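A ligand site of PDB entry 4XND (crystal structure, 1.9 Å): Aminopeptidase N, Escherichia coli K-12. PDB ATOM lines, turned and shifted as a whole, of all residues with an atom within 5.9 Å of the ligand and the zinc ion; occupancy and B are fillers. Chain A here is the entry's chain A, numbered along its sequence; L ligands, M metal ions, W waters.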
ATOM      1  N   GLU A 103      20.267 -18.661 -30.293  1.00  0.00           N
ATOM      2  CA  GLU A 103      19.586 -19.778 -29.645  1.00  0.00           C
ATOM      3  C   GLU A 103      20.701 -20.753 -29.259  1.00  0.00           C
ATOM      4  O   GLU A 103      21.515 -21.125 -30.100  1.00  0.00           O
ATOM      5  CB  GLU A 103      18.513 -20.473 -30.553  1.00  0.00           C
ATOM      6  CG  GLU A 103      17.803 -21.707 -29.883  1.00  0.00           C
ATOM      7  CD  GLU A 103      16.507 -22.215 -30.553  1.00  0.00           C
ATOM      8  OE1 GLU A 103      16.671 -22.876 -31.563  1.00  0.00           O
ATOM      9  OE2 GLU A 103      15.375 -22.013 -30.025  1.00  0.00           O
ATOM     10  N   GLN A 115      20.433 -18.789 -24.607  1.00  0.00           N
ATOM     11  CA  GLN A 115      18.982 -18.781 -24.537  1.00  0.00           C
ATOM     12  C   GLN A 115      18.507 -20.185 -24.884  1.00  0.00           C
ATOM     13  O   GLN A 115      18.807 -20.665 -26.019  1.00  0.00           O
ATOM     14  CB  GLN A 115      18.432 -17.752 -25.553  1.00  0.00           C
ATOM     15  CG  GLN A 115      16.898 -17.802 -25.696  1.00  0.00           C
ATOM     16  CD  GLN A 115      16.174 -17.617 -24.394  1.00  0.00           C
ATOM     17  OE1 GLN A 115      16.647 -16.889 -23.501  1.00  0.00           O
ATOM     18  NE2 GLN A 115      15.036 -18.280 -24.250  1.00  0.00           N
ATOM     19  N   GLU A 117      15.090 -21.501 -24.007  1.00  0.00           N
ATOM     20  CA  GLU A 117      13.630 -21.683 -24.271  1.00  0.00           C
ATOM     21  C   GLU A 117      13.414 -21.324 -25.742  1.00  0.00           C
ATOM     22  O   GLU A 117      14.030 -20.372 -26.223  1.00  0.00           O
ATOM     23  CB  GLU A 117      12.798 -20.856 -23.356  1.00  0.00           C
ATOM     24  CG  GLU A 117      11.317 -21.250 -23.390  1.00  0.00           C
ATOM     25  CD  GLU A 117      10.384 -20.493 -22.485  1.00  0.00           C
ATOM     26  OE1 GLU A 117      10.853 -19.771 -21.578  1.00  0.00           O
ATOM     27  OE2 GLU A 117       9.135 -20.713 -22.581  1.00  0.00           O
ATOM     28  N   ALA A 118      12.642 -22.123 -26.486  1.00  0.00           N
ATOM     29  CA  ALA A 118      11.960 -23.344 -25.999  1.00  0.00           C
ATOM     30  C   ALA A 118      12.868 -24.561 -26.093  1.00  0.00           C
ATOM     31  O   ALA A 118      12.916 -25.382 -25.142  1.00  0.00           O
ATOM     32  CB  ALA A 118      10.716 -23.624 -26.845  1.00  0.00           C
ATOM     33  N   TYR A 181      15.166 -26.004 -20.480  1.00  0.00           N
ATOM     34  CA  TYR A 181      14.960 -24.715 -21.098  1.00  0.00           C
ATOM     35  C   TYR A 181      15.294 -23.625 -20.060  1.00  0.00           C
ATOM     36  O   TYR A 181      15.395 -22.446 -20.428  1.00  0.00           O
ATOM     37  CB  TYR A 181      13.516 -24.506 -21.598  1.00  0.00           C
ATOM     38  CG  TYR A 181      12.435 -24.244 -20.582  1.00  0.00           C
ATOM     39  CD1 TYR A 181      12.145 -22.915 -20.157  1.00  0.00           C
ATOM     40  CD2 TYR A 181      11.647 -25.253 -20.068  1.00  0.00           C
ATOM     41  CE1 TYR A 181      11.048 -22.676 -19.329  1.00  0.00           C
ATOM     42  CE2 TYR A 181      10.633 -25.003 -19.118  1.00  0.00           C
ATOM     43  CZ  TYR A 181      10.349 -23.695 -18.748  1.00  0.00           C
ATOM     44  OH  TYR A 181       9.353 -23.418 -17.861  1.00  0.00           O
ATOM     45  N   PHE A 254      19.643 -10.128 -27.955  1.00  0.00           N
ATOM     46  CA  PHE A 254      18.647 -11.020 -27.370  1.00  0.00           C
ATOM     47  C   PHE A 254      17.395 -10.891 -28.214  1.00  0.00           C
ATOM     48  O   PHE A 254      16.933  -9.782 -28.479  1.00  0.00           O
ATOM     49  CB  PHE A 254      18.354 -10.525 -25.927  1.00  0.00           C
ATOM     50  CG  PHE A 254      17.774 -11.568 -25.056  1.00  0.00           C
ATOM     51  CD1 PHE A 254      18.553 -12.590 -24.614  1.00  0.00           C
ATOM     52  CD2 PHE A 254      16.398 -11.578 -24.769  1.00  0.00           C
ATOM     53  CE1 PHE A 254      18.068 -13.593 -23.812  1.00  0.00           C
ATOM     54  CE2 PHE A 254      15.892 -12.602 -23.965  1.00  0.00           C
ATOM     55  CZ  PHE A 254      16.733 -13.587 -23.451  1.00  0.00           C
ATOM     56  N   ASN A 255      16.845 -12.033 -28.606  1.00  0.00           N
ATOM     57  CA  ASN A 255      15.670 -12.039 -29.470  1.00  0.00           C
ATOM     58  C   ASN A 255      14.364 -11.554 -28.856  1.00  0.00           C
ATOM     59  O   ASN A 255      13.577 -10.914 -29.553  1.00  0.00           O
ATOM     60  CB  ASN A 255      15.481 -13.420 -30.076  1.00  0.00           C
ATOM     61  CG  ASN A 255      16.476 -13.723 -31.148  1.00  0.00           C
ATOM     62  OD1 ASN A 255      17.016 -12.804 -31.781  1.00  0.00           O
ATOM     63  ND2 ASN A 255      16.748 -15.005 -31.376  1.00  0.00           N
ATOM     64  N   MET A 256      14.086 -11.867 -27.610  1.00  0.00           N
ATOM     65  CA  MET A 256      12.840 -11.393 -27.016  1.00  0.00           C
ATOM     66  C   MET A 256      13.114 -10.338 -25.930  1.00  0.00           C
ATOM     67  O   MET A 256      14.115  -9.657 -26.025  1.00  0.00           O
ATOM     68  CB  MET A 256      12.130 -12.597 -26.436  1.00  0.00           C
ATOM     69  CG  MET A 256      11.774 -13.594 -27.528  1.00  0.00           C
ATOM     70  SD  MET A 256      10.224 -13.183 -28.296  1.00  0.00           S
ATOM     71  CE  MET A 256       9.246 -14.119 -27.126  1.00  0.00           C
ATOM     72  N   GLY A 257      12.308 -10.278 -24.892  1.00  0.00           N
ATOM     73  CA  GLY A 257      12.498  -9.264 -23.837  1.00  0.00           C
ATOM     74  C   GLY A 257      13.409  -9.737 -22.739  1.00  0.00           C
ATOM     75  O   GLY A 257      14.306  -9.001 -22.311  1.00  0.00           O
ATOM     76  N   ALA A 258      13.144 -10.944 -22.261  1.00  0.00           N
ATOM     77  CA  ALA A 258      13.953 -11.475 -21.151  1.00  0.00           C
ATOM     78  C   ALA A 258      13.616 -12.936 -20.947  1.00  0.00           C
ATOM     79  O   ALA A 258      12.784 -13.468 -21.652  1.00  0.00           O
ATOM     80  CB  ALA A 258      13.623 -10.678 -19.877  1.00  0.00           C
ATOM     81  N   MET A 259      14.307 -13.567 -19.996  1.00  0.00           N
ATOM     82  CA  MET A 259      14.151 -14.996 -19.818  1.00  0.00           C
ATOM     83  C   MET A 259      14.331 -15.410 -18.339  1.00  0.00           C
ATOM     84  O   MET A 259      15.344 -15.011 -17.736  1.00  0.00           O
ATOM     85  CB  MET A 259      15.139 -15.737 -20.725  1.00  0.00           C
ATOM     86  CG  MET A 259      15.172 -17.257 -20.525  1.00  0.00           C
ATOM     87  SD  MET A 259      13.600 -18.001 -21.004  1.00  0.00           S
ATOM     88  CE  MET A 259      13.469 -19.314 -19.816  1.00  0.00           C
ATOM     89  N   GLU A 260      13.368 -16.201 -17.814  1.00  0.00           N
ATOM     90  CA  GLU A 260      13.290 -16.513 -16.411  1.00  0.00           C
ATOM     91  C   GLU A 260      14.230 -17.634 -15.919  1.00  0.00           C
ATOM     92  O   GLU A 260      13.871 -18.386 -15.026  1.00  0.00           O
ATOM     93  CB  GLU A 260      11.857 -16.834 -16.055  1.00  0.00           C
ATOM     94  CG  GLU A 260      11.347 -18.149 -16.713  1.00  0.00           C
ATOM     95  CD  GLU A 260      10.577 -17.963 -18.050  1.00  0.00           C
ATOM     96  OE1 GLU A 260      10.838 -16.997 -18.826  1.00  0.00           O
ATOM     97  OE2 GLU A 260       9.749 -18.910 -18.373  1.00  0.00           O
ATOM     98  N   HIS A 293       7.619  -9.668 -14.413  1.00  0.00           N
ATOM     99  CA  HIS A 293       7.226 -10.852 -15.198  1.00  0.00           C
ATOM    100  C   HIS A 293       8.239 -11.962 -14.974  1.00  0.00           C
ATOM    101  O   HIS A 293       7.853 -13.080 -14.658  1.00  0.00           O
ATOM    102  CB  HIS A 293       7.182 -10.485 -16.714  1.00  0.00           C
ATOM    103  CG  HIS A 293       6.674 -11.587 -17.575  1.00  0.00           C
ATOM    104  ND1 HIS A 293       5.347 -11.728 -17.920  1.00  0.00           N
ATOM    105  CD2 HIS A 293       7.327 -12.611 -18.146  1.00  0.00           C
ATOM    106  CE1 HIS A 293       5.218 -12.842 -18.621  1.00  0.00           C
ATOM    107  NE2 HIS A 293       6.412 -13.389 -18.770  1.00  0.00           N
ATOM    108  N   GLU A 294       9.512 -11.696 -15.160  1.00  0.00           N
ATOM    109  CA  GLU A 294      10.539 -12.807 -15.012  1.00  0.00           C
ATOM    110  C   GLU A 294      10.618 -13.307 -13.604  1.00  0.00           C
ATOM    111  O   GLU A 294      10.726 -14.513 -13.364  1.00  0.00           O
ATOM    112  CB  GLU A 294      11.921 -12.362 -15.504  1.00  0.00           C
ATOM    113  CG  GLU A 294      11.940 -11.711 -16.909  1.00  0.00           C
ATOM    114  CD  GLU A 294      11.246 -12.559 -17.983  1.00  0.00           C
ATOM    115  OE1 GLU A 294      11.257 -13.813 -17.876  1.00  0.00           O
ATOM    116  OE2 GLU A 294      10.621 -11.935 -18.864  1.00  0.00           O
ATOM    117  N   HIS A 297       7.676 -15.642 -12.792  1.00  0.00           N
ATOM    118  CA  HIS A 297       7.903 -16.955 -13.377  1.00  0.00           C
ATOM    119  C   HIS A 297       8.583 -17.905 -12.380  1.00  0.00           C
ATOM    120  O   HIS A 297       8.544 -19.130 -12.567  1.00  0.00           O
ATOM    121  CB  HIS A 297       8.762 -16.901 -14.614  1.00  0.00           C
ATOM    122  CG  HIS A 297       8.012 -16.759 -15.908  1.00  0.00           C
ATOM    123  ND1 HIS A 297       6.978 -17.604 -16.276  1.00  0.00           N
ATOM    124  CD2 HIS A 297       8.252 -15.959 -16.972  1.00  0.00           C
ATOM    125  CE1 HIS A 297       6.633 -17.324 -17.531  1.00  0.00           C
ATOM    126  NE2 HIS A 297       7.344 -16.309 -17.937  1.00  0.00           N
ATOM    127  N   LYS A 315       2.069 -21.215 -18.053  1.00  0.00           N
ATOM    128  CA  LYS A 315       2.982 -20.261 -17.452  1.00  0.00           C
ATOM    129  C   LYS A 315       2.835 -18.826 -18.018  1.00  0.00           C
ATOM    130  O   LYS A 315       2.977 -17.887 -17.275  1.00  0.00           O
ATOM    131  CB  LYS A 315       4.478 -20.689 -17.462  1.00  0.00           C
ATOM    132  CG  LYS A 315       5.239 -20.797 -18.800  1.00  0.00           C
ATOM    133  CD  LYS A 315       6.635 -21.342 -18.594  1.00  0.00           C
ATOM    134  CE  LYS A 315       7.477 -21.371 -19.838  1.00  0.00           C
ATOM    135  NZ  LYS A 315       7.967 -20.052 -20.288  1.00  0.00           N
ATOM    136  N   GLU A 316       2.646 -18.693 -19.338  1.00  0.00           N
ATOM    137  CA  GLU A 316       2.622 -17.365 -19.899  1.00  0.00           C
ATOM    138  C   GLU A 316       1.345 -16.561 -19.635  1.00  0.00           C
ATOM    139  O   GLU A 316       1.431 -15.399 -19.249  1.00  0.00           O
ATOM    140  CB  GLU A 316       3.035 -17.331 -21.375  1.00  0.00           C
ATOM    141  CG  GLU A 316       4.474 -17.890 -21.668  1.00  0.00           C
ATOM    142  CD  GLU A 316       5.543 -17.174 -20.878  1.00  0.00           C
ATOM    143  OE1 GLU A 316       5.282 -16.084 -20.324  1.00  0.00           O
ATOM    144  OE2 GLU A 316       6.635 -17.744 -20.772  1.00  0.00           O
ATOM    145  N   THR A 319       1.511 -15.806 -15.863  1.00  0.00           N
ATOM    146  CA  THR A 319       2.568 -14.823 -15.541  1.00  0.00           C
ATOM    147  C   THR A 319       2.303 -13.461 -16.106  1.00  0.00           C
ATOM    148  O   THR A 319       2.555 -12.466 -15.422  1.00  0.00           O
ATOM    149  CB  THR A 319       3.975 -15.366 -15.884  1.00  0.00           C
ATOM    150  OG1 THR A 319       4.140 -16.664 -15.257  1.00  0.00           O
ATOM    151  CG2 THR A 319       5.075 -14.397 -15.494  1.00  0.00           C
ATOM    152  N   VAL A 320       1.696 -13.386 -17.296  1.00  0.00           N
ATOM    153  CA  VAL A 320       1.210 -12.067 -17.748  1.00  0.00           C
ATOM    154  C   VAL A 320       0.127 -11.518 -16.828  1.00  0.00           C
ATOM    155  O   VAL A 320       0.154 -10.307 -16.508  1.00  0.00           O
ATOM    156  CB  VAL A 320       0.744 -12.143 -19.207  1.00  0.00           C
ATOM    157  CG1 VAL A 320       0.066 -10.795 -19.620  1.00  0.00           C
ATOM    158  CG2 VAL A 320       1.927 -12.424 -20.116  1.00  0.00           C
ATOM    159  N   ASN A 369       8.942 -21.773 -31.534  1.00  0.00           N
ATOM    160  CA  ASN A 369       9.219 -20.356 -31.378  1.00  0.00           C
ATOM    161  C   ASN A 369       8.181 -19.419 -31.995  1.00  0.00           C
ATOM    162  O   ASN A 369       8.037 -18.258 -31.561  1.00  0.00           O
ATOM    163  CB  ASN A 369      10.617 -20.022 -31.848  1.00  0.00           C
ATOM    164  CG  ASN A 369      11.699 -20.643 -30.891  1.00  0.00           C
ATOM    165  OD1 ASN A 369      11.423 -21.123 -29.815  1.00  0.00           O
ATOM    166  ND2 ASN A 369      12.913 -20.603 -31.343  1.00  0.00           N
ATOM    167  N   TYR A 372       5.099 -18.041 -29.227  1.00  0.00           N
ATOM    168  CA  TYR A 372       5.250 -17.028 -28.160  1.00  0.00           C
ATOM    169  C   TYR A 372       4.425 -15.795 -28.590  1.00  0.00           C
ATOM    170  O   TYR A 372       4.998 -14.809 -29.037  1.00  0.00           O
ATOM    171  CB  TYR A 372       6.739 -16.760 -27.948  1.00  0.00           C
ATOM    172  CG  TYR A 372       7.311 -17.986 -27.212  1.00  0.00           C
ATOM    173  CD1 TYR A 372       7.624 -19.187 -27.901  1.00  0.00           C
ATOM    174  CD2 TYR A 372       7.439 -17.988 -25.846  1.00  0.00           C
ATOM    175  CE1 TYR A 372       8.083 -20.299 -27.212  1.00  0.00           C
ATOM    176  CE2 TYR A 372       7.896 -19.090 -25.177  1.00  0.00           C
ATOM    177  CZ  TYR A 372       8.185 -20.281 -25.884  1.00  0.00           C
ATOM    178  OH  TYR A 372       8.609 -21.406 -25.179  1.00  0.00           O
ATOM    179  N   TYR A 377       0.023 -15.317 -24.705  1.00  0.00           N
ATOM    180  CA  TYR A 377       0.326 -14.358 -23.611  1.00  0.00           C
ATOM    181  C   TYR A 377      -0.868 -13.508 -23.180  1.00  0.00           C
ATOM    182  O   TYR A 377      -1.364 -13.625 -22.036  1.00  0.00           O
ATOM    183  CB  TYR A 377       1.489 -13.439 -23.990  1.00  0.00           C
ATOM    184  CG  TYR A 377       2.886 -14.026 -23.888  1.00  0.00           C
ATOM    185  CD1 TYR A 377       3.286 -15.097 -24.696  1.00  0.00           C
ATOM    186  CD2 TYR A 377       3.809 -13.520 -22.980  1.00  0.00           C
ATOM    187  CE1 TYR A 377       4.577 -15.602 -24.597  1.00  0.00           C
ATOM    188  CE2 TYR A 377       5.103 -13.998 -22.869  1.00  0.00           C
ATOM    189  CZ  TYR A 377       5.481 -15.085 -23.658  1.00  0.00           C
ATOM    190  OH  TYR A 377       6.753 -15.630 -23.541  1.00  0.00           O
ATOM    191  N   GLN A 817      14.135 -16.506 -35.951  1.00  0.00           N
ATOM    192  CA  GLN A 817      13.154 -16.031 -34.994  1.00  0.00           C
ATOM    193  C   GLN A 817      12.756 -14.581 -35.250  1.00  0.00           C
ATOM    194  O   GLN A 817      11.586 -14.204 -35.197  1.00  0.00           O
ATOM    195  CB  GLN A 817      13.760 -16.162 -33.583  1.00  0.00           C
ATOM    196  CG  GLN A 817      12.788 -16.070 -32.443  1.00  0.00           C
ATOM    197  CD  GLN A 817      12.458 -14.630 -31.984  1.00  0.00           C
ATOM    198  OE1 GLN A 817      13.053 -13.618 -32.445  1.00  0.00           O
ATOM    199  NE2 GLN A 817      11.507 -14.533 -31.080  1.00  0.00           N
HETATM  200  N1  LIG L   1       9.826 -17.251 -21.175  1.00  0.00           N
HETATM  201  C1  LIG L   1      10.629 -16.378 -22.104  1.00  0.00           C
HETATM  202  C2  LIG L   1      10.630 -17.012 -23.517  1.00  0.00           C
HETATM  203  C3  LIG L   1      11.722 -16.604 -24.481  1.00  0.00           C
HETATM  204  C4  LIG L   1      11.891 -17.113 -25.782  1.00  0.00           C
HETATM  205  C5  LIG L   1      11.229 -18.133 -26.509  1.00  0.00           C
HETATM  206  C6  LIG L   1      11.669 -18.451 -27.823  1.00  0.00           C
HETATM  207  C7  LIG L   1      12.762 -17.778 -28.393  1.00  0.00           C
HETATM  208  C8  LIG L   1      13.441 -16.801 -27.649  1.00  0.00           C
HETATM  209  C9  LIG L   1      13.005 -16.487 -26.327  1.00  0.00           C
HETATM  210  N2  LIG L   1      13.501 -15.609 -25.380  1.00  0.00           N
HETATM  211  C10 LIG L   1      12.727 -15.650 -24.273  1.00  0.00           C
HETATM  212  C11 LIG L   1      10.108 -14.920 -22.193  1.00  0.00           C
HETATM  213  C12 LIG L   1       9.119 -14.698 -21.090  1.00  0.00           C
HETATM  214  O1  LIG L   1       7.830 -14.985 -21.170  1.00  0.00           O
HETATM  215  O2  LIG L   1       9.425 -14.402 -19.947  1.00  0.00           O
HETATM  216 ZN    ZN M   1       6.834 -15.187 -19.590  1.00  0.00          ZN
HETATM  217  O   HOH W   1       9.921 -16.699 -30.164  1.00  0.00           O
HETATM  218  O   HOH W   2      15.932 -14.497 -26.615  1.00  0.00           O
HETATM  219  O   HOH W   3      16.479 -17.242 -29.220  1.00  0.00           O
HETATM  220  O   HOH W   4      15.421 -19.776 -28.504  1.00  0.00           O
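Tyr 377 touches the zinc ion (CE2 to ZN, 3.9 Å).
Met 256 touches the ligand. O of Ala 258 touches C11 of the ligand, at 3.1 Å. SD of Met 259 touches C1 of the ligand (3.6 Å). OD1 of Asn 369 touches C6 of the ligand, at 3.3 Å. Tyr 372 touches the ligand. Hydrophobic or aromatic side chains that line the ligand: Met 256, Met 259, His 293, His 297, Tyr 372 and Tyr 377. Within 4 Å of the ligand: Gln 115, Glu 117, Met 256, Ala 258, Met 259, Glu 260, His 293, Glu 294, His 297, Lys 315, Glu 316, Asn 369, Tyr 372 and Tyr 377.
Water W4 lies within hydrogen-bond range of the side-chain carboxylate of Glu 103 and the backbone carbonyl oxygen of Glu 117. Water W1 lies within hydrogen-bond range of O of Asn 369 (2.8 Å) and NE2 of Gln 817 (2.8 Å).
The zinc ion is bound by O1 of the ligand (1.9 Å), OE1 of Glu 316 (1.9 Å), NE2 of His 293 (2.0 Å) and NE2 of His 297 (2.1 Å). The zinc ion has four donor atoms within binding distance. Slightly farther from the zinc ion lies an oxygen (O2) of the ligand (2.7 Å). Slightly farther from the zinc ion lies OE2 of Glu 316 (2.8 Å).
The side-chain carboxylate (OE2) of Glu 316 is in salt-bridge range of the side-chain amino group (NZ) of Lys 315, at 2.7 Å. The side-chain carboxylate (OE2) of Glu 103 lies within hydrogen-bond range of the side-chain amide nitrogen (ND2) of Asn 369 (3.1 Å). The side-chain carboxylate (OE2) of Glu 316 lies close to the side-chain hydroxyl (OH) of Tyr 377 (3.5 Å). OE1 of Glu 294 is in hydrogen-bond range of N of Glu 260 (3.2 Å). The side-chain hydroxyl (OG1) of Thr 319 sits at hydrogen-bond distance from a ring nitrogen (ND1) of His 297 (3.2 Å). The side-chain amide nitrogen (NE2) of Gln 115 sits at hydrogen-bond distance from the side-chain sulfur (SD) of Met 259. The backbone carbonyl oxygen (O) of Lys 315 is in hydrogen-bond range of the side-chain hydroxyl (OG1) of Thr 319, 2.6 Å away. The side-chain carboxylate (OE2) of Glu 260 lies within salt-bridge range of the side-chain amino group (NZ) of Lys 315.
OE1 of Glu 294 sits close to O2 of the ligand (2.8 Å). The side-chain carboxylate (OE1) of Glu 260 lies within salt-bridge range of a nitrogen (N1) of the ligand (2.6 Å). A nitrogen (N1) of the ligand sits close to the side-chain amino group (NZ) of Lys 315 (3.5 Å). NE2 of Gln 115 lies close to N2 of the ligand (3.3 Å). OH of Tyr 377 sits close to O1 of the ligand (2.7 Å). A nitrogen (N1) of the ligand is in salt-bridge range of the side-chain carboxylate (OE1) of Glu 117 (2.8 Å).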
